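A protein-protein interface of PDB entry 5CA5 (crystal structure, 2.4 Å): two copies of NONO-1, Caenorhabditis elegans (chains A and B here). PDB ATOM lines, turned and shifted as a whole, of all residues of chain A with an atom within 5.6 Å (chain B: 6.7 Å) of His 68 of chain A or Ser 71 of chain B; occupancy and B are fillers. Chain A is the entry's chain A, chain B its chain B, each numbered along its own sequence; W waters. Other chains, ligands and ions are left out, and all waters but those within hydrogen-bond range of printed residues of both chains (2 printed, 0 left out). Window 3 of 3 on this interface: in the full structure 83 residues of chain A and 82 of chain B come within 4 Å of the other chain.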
ATOM      1  N   HIS A  45      30.294  33.778 -23.123  1.00  0.00           N
ATOM      2  CA  HIS A  45      29.780  32.689 -23.956  1.00  0.00           C
ATOM      3  C   HIS A  45      29.161  33.123 -25.273  1.00  0.00           C
ATOM      4  O   HIS A  45      29.185  32.361 -26.232  1.00  0.00           O
ATOM      5  CB  HIS A  45      28.857  31.789 -23.134  1.00  0.00           C
ATOM      6  CG  HIS A  45      29.524  31.335 -21.876  1.00  0.00           C
ATOM      7  ND1 HIS A  45      30.436  30.295 -21.880  1.00  0.00           N
ATOM      8  CD2 HIS A  45      29.449  31.844 -20.625  1.00  0.00           C
ATOM      9  CE1 HIS A  45      30.849  30.176 -20.627  1.00  0.00           C
ATOM     10  NE2 HIS A  45      30.288  31.086 -19.839  1.00  0.00           N
ATOM     11  N   GLY A  46      28.655  34.350 -25.316  1.00  0.00           N
ATOM     12  CA  GLY A  46      28.049  34.930 -26.506  1.00  0.00           C
ATOM     13  C   GLY A  46      27.151  36.120 -26.232  1.00  0.00           C
ATOM     14  O   GLY A  46      27.011  36.574 -25.092  1.00  0.00           O
ATOM     15  N   ASP A  47      26.550  36.639 -27.309  1.00  0.00           N
ATOM     16  CA  ASP A  47      25.617  37.758 -27.291  1.00  0.00           C
ATOM     17  C   ASP A  47      24.314  37.335 -26.614  1.00  0.00           C
ATOM     18  O   ASP A  47      23.940  36.165 -26.722  1.00  0.00           O
ATOM     19  CB  ASP A  47      25.384  38.270 -28.727  1.00  0.00           C
ATOM     20  CG  ASP A  47      26.631  38.843 -29.375  1.00  0.00           C
ATOM     21  OD1 ASP A  47      27.522  39.336 -28.633  1.00  0.00           O
ATOM     22  OD2 ASP A  47      26.710  38.824 -30.628  1.00  0.00           O
ATOM     23  N   LEU A  63      21.017  33.154 -25.270  1.00  0.00           N
ATOM     24  CA  LEU A  63      22.301  33.331 -25.955  1.00  0.00           C
ATOM     25  C   LEU A  63      21.941  33.333 -27.462  1.00  0.00           C
ATOM     26  O   LEU A  63      20.847  32.886 -27.810  1.00  0.00           O
ATOM     27  CB  LEU A  63      23.300  32.181 -25.629  1.00  0.00           C
ATOM     28  CG  LEU A  63      24.250  32.301 -24.396  1.00  0.00           C
ATOM     29  CD1 LEU A  63      25.410  33.204 -24.646  1.00  0.00           C
ATOM     30  CD2 LEU A  63      23.517  32.690 -23.124  1.00  0.00           C
ATOM     31  N   ASP A  64      22.834  33.838 -28.339  1.00  0.00           N
ATOM     32  CA  ASP A  64      22.607  33.901 -29.786  1.00  0.00           C
ATOM     33  C   ASP A  64      22.433  32.550 -30.494  1.00  0.00           C
ATOM     34  O   ASP A  64      21.653  32.460 -31.455  1.00  0.00           O
ATOM     35  CB  ASP A  64      23.651  34.789 -30.475  1.00  0.00           C
ATOM     36  CG  ASP A  64      25.066  34.347 -30.268  1.00  0.00           C
ATOM     37  OD1 ASP A  64      25.392  33.914 -29.144  1.00  0.00           O
ATOM     38  OD2 ASP A  64      25.853  34.429 -31.228  1.00  0.00           O
ATOM     39  N   THR A  65      23.176  31.505 -30.030  1.00  0.00           N
ATOM     40  CA  THR A  65      23.133  30.145 -30.596  1.00  0.00           C
ATOM     41  C   THR A  65      23.021  29.118 -29.465  1.00  0.00           C
ATOM     42  O   THR A  65      23.478  29.397 -28.351  1.00  0.00           O
ATOM     43  CB  THR A  65      24.333  29.859 -31.518  1.00  0.00           C
ATOM     44  OG1 THR A  65      25.515  29.741 -30.741  1.00  0.00           O
ATOM     45  CG2 THR A  65      24.531  30.903 -32.605  1.00  0.00           C
ATOM     46  N   ARG A  66      22.431  27.928 -29.767  1.00  0.00           N
ATOM     47  CA  ARG A  66      22.254  26.811 -28.835  1.00  0.00           C
ATOM     48  C   ARG A  66      23.602  26.357 -28.290  1.00  0.00           C
ATOM     49  O   ARG A  66      23.704  26.048 -27.098  1.00  0.00           O
ATOM     50  CB  ARG A  66      21.501  25.645 -29.503  1.00  0.00           C
ATOM     51  CG  ARG A  66      21.707  24.287 -28.812  1.00  0.00           C
ATOM     52  CD  ARG A  66      20.613  23.278 -29.076  1.00  0.00           C
ATOM     53  NE  ARG A  66      19.582  23.247 -28.027  1.00  0.00           N
ATOM     54  CZ  ARG A  66      19.652  22.550 -26.893  1.00  0.00           C
ATOM     55  NH1 ARG A  66      20.715  21.798 -26.630  1.00  0.00           N
ATOM     56  NH2 ARG A  66      18.651  22.582 -26.028  1.00  0.00           N
ATOM     57  N   ALA A  67      24.636  26.376 -29.155  1.00  0.00           N
ATOM     58  CA  ALA A  67      26.023  26.033 -28.838  1.00  0.00           C
ATOM     59  C   ALA A  67      26.629  26.996 -27.798  1.00  0.00           C
ATOM     60  O   ALA A  67      27.336  26.530 -26.902  1.00  0.00           O
ATOM     61  CB  ALA A  67      26.864  26.016 -30.110  1.00  0.00           C
ATOM     62  N   HIS A  68      26.312  28.318 -27.883  1.00  0.00           N
ATOM     63  CA  HIS A  68      26.782  29.325 -26.913  1.00  0.00           C
ATOM     64  C   HIS A  68      26.072  29.206 -25.571  1.00  0.00           C
ATOM     65  O   HIS A  68      26.656  29.510 -24.523  1.00  0.00           O
ATOM     66  CB  HIS A  68      26.628  30.749 -27.470  1.00  0.00           C
ATOM     67  CG  HIS A  68      27.559  31.036 -28.596  1.00  0.00           C
ATOM     68  ND1 HIS A  68      27.301  32.042 -29.500  1.00  0.00           N
ATOM     69  CD2 HIS A  68      28.715  30.421 -28.940  1.00  0.00           C
ATOM     70  CE1 HIS A  68      28.302  32.012 -30.365  1.00  0.00           C
ATOM     71  NE2 HIS A  68      29.172  31.044 -30.072  1.00  0.00           N
ATOM     72  N   ALA A  69      24.796  28.771 -25.635  1.00  0.00           N
ATOM     73  CA  ALA A  69      23.870  28.537 -24.527  1.00  0.00           C
ATOM     74  C   ALA A  69      24.225  27.253 -23.765  1.00  0.00           C
ATOM     75  O   ALA A  69      24.058  27.217 -22.541  1.00  0.00           O
ATOM     76  CB  ALA A  69      22.437  28.487 -25.053  1.00  0.00           C
ATOM     77  N   GLU A  70      24.732  26.208 -24.483  1.00  0.00           N
ATOM     78  CA  GLU A  70      25.182  24.932 -23.893  1.00  0.00           C
ATOM     79  C   GLU A  70      26.480  25.163 -23.142  1.00  0.00           C
ATOM     80  O   GLU A  70      26.641  24.691 -22.025  1.00  0.00           O
ATOM     81  CB  GLU A  70      25.385  23.875 -24.972  1.00  0.00           C
ATOM     82  CG  GLU A  70      24.831  22.513 -24.596  1.00  0.00           C
ATOM     83  CD  GLU A  70      24.574  21.611 -25.793  1.00  0.00           C
ATOM     84  OE1 GLU A  70      25.331  20.625 -25.951  1.00  0.00           O
ATOM     85  OE2 GLU A  70      23.646  21.899 -26.587  1.00  0.00           O
ATOM     86  N   SER A  71      27.364  25.964 -23.734  1.00  0.00           N
ATOM     87  CA  SER A  71      28.653  26.383 -23.195  1.00  0.00           C
ATOM     88  C   SER A  71      28.457  27.227 -21.934  1.00  0.00           C
ATOM     89  O   SER A  71      29.179  27.029 -20.971  1.00  0.00           O
ATOM     90  CB  SER A  71      29.439  27.136 -24.269  1.00  0.00           C
ATOM     91  OG  SER A  71      30.549  27.839 -23.742  1.00  0.00           O
ATOM     92  N   ALA A  72      27.470  28.149 -21.937  1.00  0.00           N
ATOM     93  CA  ALA A  72      27.118  29.013 -20.793  1.00  0.00           C
ATOM     94  C   ALA A  72      26.560  28.176 -19.638  1.00  0.00           C
ATOM     95  O   ALA A  72      26.957  28.387 -18.489  1.00  0.00           O
ATOM     96  CB  ALA A  72      26.109  30.077 -21.215  1.00  0.00           C
ATOM     97  N   LYS A  73      25.701  27.186 -19.959  1.00  0.00           N
ATOM     98  CA  LYS A  73      25.081  26.256 -19.015  1.00  0.00           C
ATOM     99  C   LYS A  73      26.133  25.416 -18.311  1.00  0.00           C
ATOM    100  O   LYS A  73      26.142  25.319 -17.079  1.00  0.00           O
ATOM    101  CB  LYS A  73      24.060  25.360 -19.759  1.00  0.00           C
ATOM    102  CG  LYS A  73      23.452  24.228 -18.941  1.00  0.00           C
ATOM    103  CD  LYS A  73      22.864  23.216 -19.874  1.00  0.00           C
ATOM    104  CE  LYS A  73      22.397  21.984 -19.172  1.00  0.00           C
ATOM    105  NZ  LYS A  73      20.935  21.824 -19.361  1.00  0.00           N
ATOM    106  N   PRO B  44      39.475  30.937 -30.759  1.00  0.00           N
ATOM    107  CA  PRO B  44      38.368  31.748 -30.204  1.00  0.00           C
ATOM    108  C   PRO B  44      37.197  30.935 -29.630  1.00  0.00           C
ATOM    109  O   PRO B  44      36.464  31.425 -28.789  1.00  0.00           O
ATOM    110  CB  PRO B  44      37.899  32.577 -31.416  1.00  0.00           C
ATOM    111  CG  PRO B  44      39.063  32.643 -32.314  1.00  0.00           C
ATOM    112  CD  PRO B  44      39.760  31.335 -32.161  1.00  0.00           C
ATOM    113  N   HIS B  45      37.020  29.703 -30.104  1.00  0.00           N
ATOM    114  CA  HIS B  45      35.928  28.810 -29.718  1.00  0.00           C
ATOM    115  C   HIS B  45      36.208  27.932 -28.524  1.00  0.00           C
ATOM    116  O   HIS B  45      35.276  27.575 -27.811  1.00  0.00           O
ATOM    117  CB  HIS B  45      35.459  27.997 -30.921  1.00  0.00           C
ATOM    118  CG  HIS B  45      35.159  28.878 -32.089  1.00  0.00           C
ATOM    119  ND1 HIS B  45      33.963  29.558 -32.180  1.00  0.00           N
ATOM    120  CD2 HIS B  45      35.936  29.205 -33.151  1.00  0.00           C
ATOM    121  CE1 HIS B  45      34.035  30.246 -33.308  1.00  0.00           C
ATOM    122  NE2 HIS B  45      35.206  30.066 -33.922  1.00  0.00           N
ATOM    123  N   ARG B  66      31.814  19.527 -26.952  1.00  0.00           N
ATOM    124  CA  ARG B  66      31.003  19.399 -28.167  1.00  0.00           C
ATOM    125  C   ARG B  66      30.389  20.747 -28.528  1.00  0.00           C
ATOM    126  O   ARG B  66      30.319  21.095 -29.710  1.00  0.00           O
ATOM    127  CB  ARG B  66      29.934  18.301 -28.014  1.00  0.00           C
ATOM    128  CG  ARG B  66      28.764  18.446 -28.974  1.00  0.00           C
ATOM    129  CD  ARG B  66      28.027  17.163 -29.213  1.00  0.00           C
ATOM    130  NE  ARG B  66      27.431  17.180 -30.551  1.00  0.00           N
ATOM    131  CZ  ARG B  66      27.982  16.671 -31.649  1.00  0.00           C
ATOM    132  NH1 ARG B  66      29.168  16.076 -31.592  1.00  0.00           N
ATOM    133  NH2 ARG B  66      27.347  16.747 -32.813  1.00  0.00           N
ATOM    134  N   ALA B  67      29.990  21.511 -27.496  1.00  0.00           N
ATOM    135  CA  ALA B  67      29.414  22.856 -27.604  1.00  0.00           C
ATOM    136  C   ALA B  67      30.421  23.865 -28.219  1.00  0.00           C
ATOM    137  O   ALA B  67      30.011  24.687 -29.045  1.00  0.00           O
ATOM    138  CB  ALA B  67      28.936  23.334 -26.231  1.00  0.00           C
ATOM    139  N   HIS B  68      31.733  23.764 -27.856  1.00  0.00           N
ATOM    140  CA  HIS B  68      32.793  24.620 -28.419  1.00  0.00           C
ATOM    141  C   HIS B  68      33.134  24.257 -29.863  1.00  0.00           C
ATOM    142  O   HIS B  68      33.512  25.126 -30.659  1.00  0.00           O
ATOM    143  CB  HIS B  68      34.052  24.578 -27.553  1.00  0.00           C
ATOM    144  CG  HIS B  68      33.873  25.234 -26.222  1.00  0.00           C
ATOM    145  ND1 HIS B  68      34.707  24.939 -25.152  1.00  0.00           N
ATOM    146  CD2 HIS B  68      32.954  26.137 -25.818  1.00  0.00           C
ATOM    147  CE1 HIS B  68      34.269  25.668 -24.145  1.00  0.00           C
ATOM    148  NE2 HIS B  68      33.213  26.397 -24.498  1.00  0.00           N
ATOM    149  N   ALA B  69      32.991  22.944 -30.174  1.00  0.00           N
ATOM    150  CA  ALA B  69      33.211  22.301 -31.469  1.00  0.00           C
ATOM    151  C   ALA B  69      32.076  22.613 -32.450  1.00  0.00           C
ATOM    152  O   ALA B  69      32.343  22.764 -33.657  1.00  0.00           O
ATOM    153  CB  ALA B  69      33.368  20.800 -31.287  1.00  0.00           C
ATOM    154  N   GLU B  70      30.817  22.739 -31.937  1.00  0.00           N
ATOM    155  CA  GLU B  70      29.636  23.110 -32.732  1.00  0.00           C
ATOM    156  C   GLU B  70      29.741  24.583 -33.124  1.00  0.00           C
ATOM    157  O   GLU B  70      29.502  24.936 -34.267  1.00  0.00           O
ATOM    158  CB  GLU B  70      28.354  22.864 -31.940  1.00  0.00           C
ATOM    159  CG  GLU B  70      27.264  22.198 -32.754  1.00  0.00           C
ATOM    160  CD  GLU B  70      26.207  21.510 -31.908  1.00  0.00           C
ATOM    161  OE1 GLU B  70      25.072  22.039 -31.859  1.00  0.00           O
ATOM    162  OE2 GLU B  70      26.515  20.467 -31.277  1.00  0.00           O
ATOM    163  N   SER B  71      30.172  25.415 -32.178  1.00  0.00           N
ATOM    164  CA  SER B  71      30.395  26.837 -32.318  1.00  0.00           C
ATOM    165  C   SER B  71      31.514  27.112 -33.334  1.00  0.00           C
ATOM    166  O   SER B  71      31.372  28.018 -34.150  1.00  0.00           O
ATOM    167  CB  SER B  71      30.719  27.441 -30.953  1.00  0.00           C
ATOM    168  OG  SER B  71      31.216  28.765 -31.045  1.00  0.00           O
ATOM    169  N   ALA B  72      32.609  26.327 -33.285  1.00  0.00           N
ATOM    170  CA  ALA B  72      33.754  26.432 -34.212  1.00  0.00           C
ATOM    171  C   ALA B  72      33.338  26.060 -35.622  1.00  0.00           C
ATOM    172  O   ALA B  72      33.703  26.773 -36.561  1.00  0.00           O
ATOM    173  CB  ALA B  72      34.903  25.549 -33.744  1.00  0.00           C
ATOM    174  N   LYS B  73      32.518  24.982 -35.758  1.00  0.00           N
ATOM    175  CA  LYS B  73      31.965  24.468 -37.013  1.00  0.00           C
ATOM    176  C   LYS B  73      31.079  25.518 -37.690  1.00  0.00           C
ATOM    177  O   LYS B  73      31.244  25.832 -38.878  1.00  0.00           O
ATOM    178  CB  LYS B  73      31.190  23.164 -36.747  1.00  0.00           C
ATOM    179  CG  LYS B  73      30.418  22.604 -37.932  1.00  0.00           C
ATOM    180  CD  LYS B  73      29.358  21.638 -37.443  1.00  0.00           C
ATOM    181  CE  LYS B  73      28.399  21.191 -38.530  1.00  0.00           C
ATOM    182  NZ  LYS B  73      27.177  22.058 -38.641  1.00  0.00           N
ATOM    183  N   GLU B  74      30.153  26.058 -36.920  1.00  0.00           N
ATOM    184  CA  GLU B  74      29.173  27.045 -37.349  1.00  0.00           C
ATOM    185  C   GLU B  74      29.797  28.381 -37.756  1.00  0.00           C
ATOM    186  O   GLU B  74      29.259  29.054 -38.642  1.00  0.00           O
ATOM    187  CB  GLU B  74      28.109  27.230 -36.258  1.00  0.00           C
ATOM    188  CG  GLU B  74      27.185  26.028 -36.106  1.00  0.00           C
ATOM    189  CD  GLU B  74      25.989  26.167 -35.181  1.00  0.00           C
ATOM    190  OE1 GLU B  74      26.061  26.944 -34.201  1.00  0.00           O
ATOM    191  OE2 GLU B  74      24.987  25.453 -35.421  1.00  0.00           O
ATOM    192  N   ALA B  75      30.914  28.778 -37.105  1.00  0.00           N
ATOM    193  CA  ALA B  75      31.584  30.049 -37.419  1.00  0.00           C
ATOM    194  C   ALA B  75      32.629  29.964 -38.544  1.00  0.00           C
ATOM    195  O   ALA B  75      32.810  30.943 -39.271  1.00  0.00           O
ATOM    196  CB  ALA B  75      32.201  30.656 -36.172  1.00  0.00           C
ATOM    197  N   ILE B  76      33.299  28.797 -38.684  1.00  0.00           N
ATOM    198  CA  ILE B  76      34.349  28.559 -39.664  1.00  0.00           C
ATOM    199  C   ILE B  76      33.901  27.845 -40.965  1.00  0.00           C
ATOM    200  O   ILE B  76      34.504  28.117 -42.003  1.00  0.00           O
ATOM    201  CB  ILE B  76      35.633  27.970 -38.979  1.00  0.00           C
ATOM    202  CG1 ILE B  76      36.045  28.831 -37.754  1.00  0.00           C
ATOM    203  CG2 ILE B  76      36.815  27.837 -39.955  1.00  0.00           C
ATOM    204  CD1 ILE B  76      36.859  28.144 -36.657  1.00  0.00           C
ATOM    205  N   PHE B  90      31.573  17.750 -38.314  1.00  0.00           N
ATOM    206  CA  PHE B  90      31.934  16.869 -37.220  1.00  0.00           C
ATOM    207  C   PHE B  90      32.401  15.584 -37.844  1.00  0.00           C
ATOM    208  O   PHE B  90      31.712  15.047 -38.715  1.00  0.00           O
ATOM    209  CB  PHE B  90      30.764  16.591 -36.247  1.00  0.00           C
ATOM    210  CG  PHE B  90      30.640  17.574 -35.110  1.00  0.00           C
ATOM    211  CD1 PHE B  90      31.357  17.395 -33.934  1.00  0.00           C
ATOM    212  CD2 PHE B  90      29.825  18.693 -35.225  1.00  0.00           C
ATOM    213  CE1 PHE B  90      31.249  18.317 -32.888  1.00  0.00           C
ATOM    214  CE2 PHE B  90      29.732  19.615 -34.189  1.00  0.00           C
ATOM    215  CZ  PHE B  90      30.414  19.402 -33.010  1.00  0.00           C
HETATM  216  O   HOH W   1      27.328  28.606 -32.334  1.00  0.00           O
HETATM  217  O   HOH W   2      32.073  25.330 -21.457  1.00  0.00           O
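Ala 67 of chain A touches Ala 67 of chain B (CB to O, 3.6 Å).
Glu 70 of chain B touches Ala 67 of chain A (CB to CB, 3.9 Å).
N of Ser 71 of chain B touches CB of Ala 67 of chain A, 3.9 Å away.
Ala 67 of chain B touches Glu 70 of chain A (CB to CB, 3.8 Å).
Ala 67 of chain B touches Ser 71 of chain A (CB to N, 3.95 Å).
Thr 65 of chain A touches none of the printed residues of chain B.
Of chain B, only Ser 71 comes within 4 Å of His 68 of chain A.
Ala 69 of chain A touches none of the printed residues of chain B.
Of the printed residues of chain A, His 68 of chain B touches Ser 71.
Of the printed residues of chain A, Glu 70 of chain B touches Ala 67 (3.9 Å).
The nearest printed residue of chain A that does not touch Ala 67 of chain B is His 68 of chain A (5.3 Å).
Of the 14 printed residues of chain B, 4 touch a printed residue of chain A.
Hydrophobic or aromatic side chains of chain B within 4 Å of the printed part of chain A: Ala 67 and His 68.
Along chain B the printed residues that touch a printed residue of chain A span positions 67 to 71.
Among the printed residues, no Asp or Glu carboxylate lies within 4 Å of a Lys or Arg side-chain nitrogen of the other chain.
The side-chain hydroxyl (OG) of Ser 71 of chain A is in hydrogen-bond range of a ring nitrogen (ND1) of His 45 of chain A (3.1 Å).
OD1 of Asp 64 of chain A is in hydrogen-bond range of ND1 of His 68 of chain A, at 2.7 Å.
The side-chain hydroxyl of Thr 65 of chain A sits at hydrogen-bond distance from a ring nitrogen (ND1) of His 68 of chain A (3.2 Å).
OE2 of Glu 70 of chain A lies within salt-bridge range of NH1 of Arg 66 of chain A.
OG of Ser 71 of chain B sits at hydrogen-bond distance from ND1 of His 45 of chain B (3.1 Å).
The guanidinium group (NE) of Arg 66 of chain B lies within salt-bridge range of the side-chain carboxylate (OE2) of Glu 70 of chain B, at 3.5 Å.
NE2 of His 68 of chain A lies within hydrogen-bond range of OG of Ser 71 of chain B, at 3.2 Å.
The side-chain hydroxyl (OG) of Ser 71 of chain A is in hydrogen-bond range of a ring nitrogen (NE2) of His 68 of chain B, 3.1 Å away.
Water W1 bridges the side-chain hydroxyl of Thr 65 of chain A (2.7 Å) and the side-chain carboxylate of Glu 74 of chain B (2.8 Å).
Water W2 lies within hydrogen-bond range of O of Ser 71 of chain A (3.4 Å) and NE2 of His 68 of chain B (3.4 Å).
Ala 67 of chain B touches its own counterpart, Ala 67 of chain A.
Ala 67 of chain A touches Glu 70 of chain B, and with the chains exchanged Glu 70 of chain A touches Ala 67 of chain B.
Ala 67 of chain A touches Ser 71 of chain B, and with the chains exchanged Ser 71 of chain A touches Ala 67 of chain B.
His 68 of chain A touches Ser 71 of chain B, and with the chains exchanged Ser 71 of chain A touches His 68 of chain B.
9 positions are printed for both chains.
Of the 7 pairs that touch across the chains among the printed residues, 7 have their exchanged pair printed and touching as well.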
